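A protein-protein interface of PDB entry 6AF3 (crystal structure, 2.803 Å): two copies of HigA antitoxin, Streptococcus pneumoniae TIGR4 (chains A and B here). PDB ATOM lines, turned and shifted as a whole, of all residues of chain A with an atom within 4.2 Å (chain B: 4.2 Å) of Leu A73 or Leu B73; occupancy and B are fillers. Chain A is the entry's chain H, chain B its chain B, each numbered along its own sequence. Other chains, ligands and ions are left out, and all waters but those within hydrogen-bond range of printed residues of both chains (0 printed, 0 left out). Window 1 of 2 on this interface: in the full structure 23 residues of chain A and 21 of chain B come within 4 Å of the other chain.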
ATOM      1  N   MET A  28      27.839   2.428  31.014  1.00  0.00           N
ATOM      2  CA  MET A  28      27.424   3.712  30.513  1.00  0.00           C
ATOM      3  C   MET A  28      25.936   3.948  30.581  1.00  0.00           C
ATOM      4  O   MET A  28      25.512   5.025  30.946  1.00  0.00           O
ATOM      5  CB  MET A  28      27.890   3.890  29.042  1.00  0.00           C
ATOM      6  CG  MET A  28      28.999   4.901  28.969  1.00  0.00           C
ATOM      7  SD  MET A  28      28.482   6.674  29.767  1.00  0.00           S
ATOM      8  CE  MET A  28      27.554   7.138  28.074  1.00  0.00           C
ATOM      9  N   SER A  70      21.841   3.240  21.847  1.00  0.00           N
ATOM     10  CA  SER A  70      22.544   4.509  22.247  1.00  0.00           C
ATOM     11  C   SER A  70      22.090   5.820  21.571  1.00  0.00           C
ATOM     12  O   SER A  70      21.911   5.867  20.337  1.00  0.00           O
ATOM     13  CB  SER A  70      24.057   4.359  22.024  1.00  0.00           C
ATOM     14  OG  SER A  70      24.315   4.158  20.641  1.00  0.00           O
ATOM     15  N   PRO A  71      21.888   6.877  22.400  1.00  0.00           N
ATOM     16  CA  PRO A  71      21.400   8.180  21.947  1.00  0.00           C
ATOM     17  C   PRO A  71      22.587   9.001  21.511  1.00  0.00           C
ATOM     18  O   PRO A  71      23.693   8.473  21.584  1.00  0.00           O
ATOM     19  CB  PRO A  71      20.712   8.768  23.187  1.00  0.00           C
ATOM     20  CG  PRO A  71      21.285   8.020  24.388  1.00  0.00           C
ATOM     21  CD  PRO A  71      22.221   6.910  23.840  1.00  0.00           C
ATOM     22  N   GLN A  72      22.403  10.224  21.038  1.00  0.00           N
ATOM     23  CA  GLN A  72      23.547  10.922  20.434  1.00  0.00           C
ATOM     24  C   GLN A  72      24.453  11.656  21.409  1.00  0.00           C
ATOM     25  O   GLN A  72      23.974  12.214  22.398  1.00  0.00           O
ATOM     26  CB  GLN A  72      23.052  11.889  19.402  1.00  0.00           C
ATOM     27  CG  GLN A  72      23.015  11.250  18.082  1.00  0.00           C
ATOM     28  CD  GLN A  72      23.296  12.246  17.021  1.00  0.00           C
ATOM     29  OE1 GLN A  72      22.983  13.430  17.182  1.00  0.00           O
ATOM     30  NE2 GLN A  72      23.900  11.796  15.920  1.00  0.00           N
ATOM     31  N   LEU A  73      25.755  11.683  21.129  1.00  0.00           N
ATOM     32  CA  LEU A  73      26.719  12.270  22.084  1.00  0.00           C
ATOM     33  C   LEU A  73      26.226  13.616  22.503  1.00  0.00           C
ATOM     34  O   LEU A  73      26.289  13.946  23.667  1.00  0.00           O
ATOM     35  CB  LEU A  73      28.164  12.391  21.523  1.00  0.00           C
ATOM     36  CG  LEU A  73      29.166  12.913  22.560  1.00  0.00           C
ATOM     37  CD1 LEU A  73      29.293  11.971  23.725  1.00  0.00           C
ATOM     38  CD2 LEU A  73      30.555  13.240  22.001  1.00  0.00           C
ATOM     39  N   ASP A  74      25.705  14.390  21.571  1.00  0.00           N
ATOM     40  CA  ASP A  74      25.261  15.738  21.917  1.00  0.00           C
ATOM     41  C   ASP A  74      24.092  15.753  22.991  1.00  0.00           C
ATOM     42  O   ASP A  74      24.250  16.257  24.153  1.00  0.00           O
ATOM     43  CB  ASP A  74      24.848  16.466  20.627  1.00  0.00           C
ATOM     44  CG  ASP A  74      23.540  15.866  19.981  1.00  0.00           C
ATOM     45  OD1 ASP A  74      23.598  14.761  19.397  1.00  0.00           O
ATOM     46  OD2 ASP A  74      22.435  16.475  20.098  1.00  0.00           O
ATOM     47  N   THR A  75      22.972  15.143  22.595  1.00  0.00           N
ATOM     48  CA  THR A  75      21.726  15.068  23.328  1.00  0.00           C
ATOM     49  C   THR A  75      21.980  14.624  24.758  1.00  0.00           C
ATOM     50  O   THR A  75      21.547  15.288  25.730  1.00  0.00           O
ATOM     51  CB  THR A  75      20.803  14.052  22.673  1.00  0.00           C
ATOM     52  OG1 THR A  75      21.275  12.734  23.001  1.00  0.00           O
ATOM     53  CG2 THR A  75      20.796  14.213  21.141  1.00  0.00           C
ATOM     54  N   VAL A  76      22.692  13.498  24.869  1.00  0.00           N
ATOM     55  CA  VAL A  76      23.235  13.063  26.146  1.00  0.00           C
ATOM     56  C   VAL A  76      23.968  14.187  26.889  1.00  0.00           C
ATOM     57  O   VAL A  76      23.795  14.278  28.081  1.00  0.00           O
ATOM     58  CB  VAL A  76      24.192  11.862  25.998  1.00  0.00           C
ATOM     59  CG1 VAL A  76      24.810  11.483  27.315  1.00  0.00           C
ATOM     60  CG2 VAL A  76      23.449  10.695  25.394  1.00  0.00           C
ATOM     61  N   LEU A  77      24.760  15.050  26.234  1.00  0.00           N
ATOM     62  CA  LEU A  77      25.489  16.050  27.013  1.00  0.00           C
ATOM     63  C   LEU A  77      24.649  17.285  27.495  1.00  0.00           C
ATOM     64  O   LEU A  77      24.944  17.818  28.555  1.00  0.00           O
ATOM     65  CB  LEU A  77      26.667  16.548  26.229  1.00  0.00           C
ATOM     66  CG  LEU A  77      28.091  16.048  26.017  1.00  0.00           C
ATOM     67  CD1 LEU A  77      28.636  17.227  25.168  1.00  0.00           C
ATOM     68  CD2 LEU A  77      28.982  15.825  27.245  1.00  0.00           C
ATOM     69  N   ILE B  32      37.605  14.086  22.067  1.00  0.00           N
ATOM     70  CA  ILE B  32      37.631  12.946  21.123  1.00  0.00           C
ATOM     71  C   ILE B  32      38.601  13.054  19.910  1.00  0.00           C
ATOM     72  O   ILE B  32      39.459  12.173  19.725  1.00  0.00           O
ATOM     73  CB  ILE B  32      36.230  12.704  20.520  1.00  0.00           C
ATOM     74  CG1 ILE B  32      35.290  12.137  21.545  1.00  0.00           C
ATOM     75  CG2 ILE B  32      36.266  11.749  19.313  1.00  0.00           C
ATOM     76  CD1 ILE B  32      33.996  11.838  20.903  1.00  0.00           C
ATOM     77  N   PRO B  71      28.163  11.828  17.090  1.00  0.00           N
ATOM     78  CA  PRO B  71      27.991  10.407  16.918  1.00  0.00           C
ATOM     79  C   PRO B  71      26.934   9.804  17.878  1.00  0.00           C
ATOM     80  O   PRO B  71      26.569  10.364  18.920  1.00  0.00           O
ATOM     81  CB  PRO B  71      29.380   9.877  17.220  1.00  0.00           C
ATOM     82  CG  PRO B  71      29.828  10.711  18.212  1.00  0.00           C
ATOM     83  CD  PRO B  71      29.226  12.070  18.050  1.00  0.00           C
ATOM     84  N   GLN B  72      26.396   8.646  17.558  1.00  0.00           N
ATOM     85  CA  GLN B  72      25.579   8.133  18.610  1.00  0.00           C
ATOM     86  C   GLN B  72      26.654   7.573  19.517  1.00  0.00           C
ATOM     87  O   GLN B  72      27.839   7.658  19.174  1.00  0.00           O
ATOM     88  CB  GLN B  72      24.476   7.158  18.156  1.00  0.00           C
ATOM     89  CG  GLN B  72      24.827   5.756  17.809  1.00  0.00           C
ATOM     90  CD  GLN B  72      23.575   5.104  17.266  1.00  0.00           C
ATOM     91  OE1 GLN B  72      22.709   5.823  16.763  1.00  0.00           O
ATOM     92  NE2 GLN B  72      23.434   3.768  17.394  1.00  0.00           N
ATOM     93  N   LEU B  73      26.250   7.065  20.682  1.00  0.00           N
ATOM     94  CA  LEU B  73      27.149   6.956  21.835  1.00  0.00           C
ATOM     95  C   LEU B  73      28.068   5.766  21.808  1.00  0.00           C
ATOM     96  O   LEU B  73      29.266   5.864  22.116  1.00  0.00           O
ATOM     97  CB  LEU B  73      26.323   6.890  23.103  1.00  0.00           C
ATOM     98  CG  LEU B  73      26.964   7.691  24.223  1.00  0.00           C
ATOM     99  CD1 LEU B  73      27.702   8.889  23.568  1.00  0.00           C
ATOM    100  CD2 LEU B  73      25.834   8.110  25.191  1.00  0.00           C
ATOM    101  N   ASP B  74      27.469   4.645  21.426  1.00  0.00           N
ATOM    102  CA  ASP B  74      28.112   3.369  21.481  1.00  0.00           C
ATOM    103  C   ASP B  74      29.380   3.414  20.678  1.00  0.00           C
ATOM    104  O   ASP B  74      30.436   2.998  21.213  1.00  0.00           O
ATOM    105  CB  ASP B  74      27.194   2.306  20.949  1.00  0.00           C
ATOM    106  CG  ASP B  74      27.055   2.395  19.459  1.00  0.00           C
ATOM    107  OD1 ASP B  74      26.833   3.546  18.981  1.00  0.00           O
ATOM    108  OD2 ASP B  74      27.285   1.360  18.770  1.00  0.00           O
ATOM    109  N   THR B  75      29.264   3.971  19.444  1.00  0.00           N
ATOM    110  CA  THR B  75      30.330   4.048  18.421  1.00  0.00           C
ATOM    111  C   THR B  75      31.565   4.623  19.030  1.00  0.00           C
ATOM    112  O   THR B  75      32.639   4.057  18.864  1.00  0.00           O
ATOM    113  CB  THR B  75      29.927   4.875  17.182  1.00  0.00           C
ATOM    114  OG1 THR B  75      28.899   5.778  17.535  1.00  0.00           O
ATOM    115  CG2 THR B  75      29.353   4.034  16.098  1.00  0.00           C
ATOM    116  N   VAL B  76      31.378   5.682  19.825  1.00  0.00           N
ATOM    117  CA  VAL B  76      32.438   6.347  20.594  1.00  0.00           C
ATOM    118  C   VAL B  76      33.049   5.483  21.653  1.00  0.00           C
ATOM    119  O   VAL B  76      34.278   5.483  21.848  1.00  0.00           O
ATOM    120  CB  VAL B  76      31.929   7.599  21.312  1.00  0.00           C
ATOM    121  CG1 VAL B  76      33.058   8.294  21.877  1.00  0.00           C
ATOM    122  CG2 VAL B  76      31.203   8.515  20.349  1.00  0.00           C
ATOM    123  N   LEU B  77      32.194   4.792  22.393  1.00  0.00           N
ATOM    124  CA  LEU B  77      32.698   3.820  23.357  1.00  0.00           C
ATOM    125  C   LEU B  77      33.615   2.780  22.663  1.00  0.00           C
ATOM    126  O   LEU B  77      34.708   2.432  23.145  1.00  0.00           O
ATOM    127  CB  LEU B  77      31.520   3.122  24.051  1.00  0.00           C
ATOM    128  CG  LEU B  77      30.704   4.156  24.803  1.00  0.00           C
ATOM    129  CD1 LEU B  77      29.673   3.496  25.698  1.00  0.00           C
ATOM    130  CD2 LEU B  77      31.666   5.065  25.580  1.00  0.00           C
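Printed residues of chain B within 4 Å of Ser A70: Gln B72 (3.3 Å), Leu B73 (3.5 Å) and Asp B74 (3.1 Å). Printed residues of chain B within 4 Å of Pro A71: Gln B72 and Leu B73. Printed residues of chain B within 4 Å of Leu A73: Ile B32 (3.9 Å), Pro B71 (2.7 Å) and Leu B73 (3.5 Å). Of the printed residues of chain A, Ile B32 touches Leu A73. Printed residues of chain A within 4 Å of Pro B71: Gln A72 and Leu A73. Of chain A, only Met A28 (3.5 Å), Ser A70 (3.5 Å), Pro A71 (3.1 Å), Leu A73 (3.5 Å) and Val A76 (3.5 Å) come within 4 Å of Leu B73. Val B76 touches none of the printed residues of chain A. Printed residues of chain A within 4 Å of Leu B77: Met A28. The nearest printed residue of chain B that does not touch Ser A70 is Thr B75 (5.1 Å).
O of Gln B72 is in hydrogen-bond range of OG1 of Thr B75 (2.7 Å). The side-chain carboxylate (OD1) of Asp B74 sits at hydrogen-bond distance from the side-chain hydroxyl (OG1) of Thr B75, at 3.4 Å. The side-chain amide oxygen of Gln A72 lies close to the side-chain carboxylate of Asp A74 (2.7 Å). O of Gln A72 sits at hydrogen-bond distance from OG1 of Thr A75 (2.8 Å).
Pro A71 touches Leu B73, and with the chains exchanged Leu A73 touches Pro B71. Gln B72 touches its own counterpart, Gln A72. Leu A73 touches its own counterpart, Leu B73. Val A76 touches Leu B73, but with the chains exchanged Leu A73 does not touch Val B76 (5.0 Å). Of the 13 pairs that touch across the chains among the printed residues, 6 have their exchanged pair printed and touching as well.
Hydrophobic or aromatic side chains of chain A within 4 Å of the printed part of chain B: Met A28, Leu A73 and Val A76. Of the 8 printed residues of chain B, 6 touch a printed residue of chain A.
Met A28 touches Leu B73 (CE to CD2, 3.5 Å). Met A28 touches Leu B77 (CG to CD1, 3.6 Å). Gln B72 touches Pro A71 (CA to O, 3.5 Å). CA of Gln A72 touches O of Pro B71, 3.4 Å away. CA of Gln A72 touches CA of Gln B72 (3.9 Å). Leu A73 touches Ile B32 (CD2 to CD1, 3.9 Å). Leu A73 touches Leu B73. Val A76 touches Leu B73 (CG2 to CD2, 3.5 Å).
The backbone NH (N) of Leu A73 lies within hydrogen-bond range of the backbone carbonyl oxygen (O) of Pro B71 (2.7 Å). The side-chain amide nitrogen (NE2) of Gln B72 lies close to the side-chain hydroxyl (OG) of Ser A70 (3.4 Å). The backbone NH (N) of Leu B73 lies within hydrogen-bond range of the side-chain hydroxyl (OG) of Ser A70, at 3.5 Å. N of Leu B73 lies within hydrogen-bond range of O of Pro A71. OD1 of Asp B74 lies within hydrogen-bond range of OG of Ser A70, 3.1 Å away.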
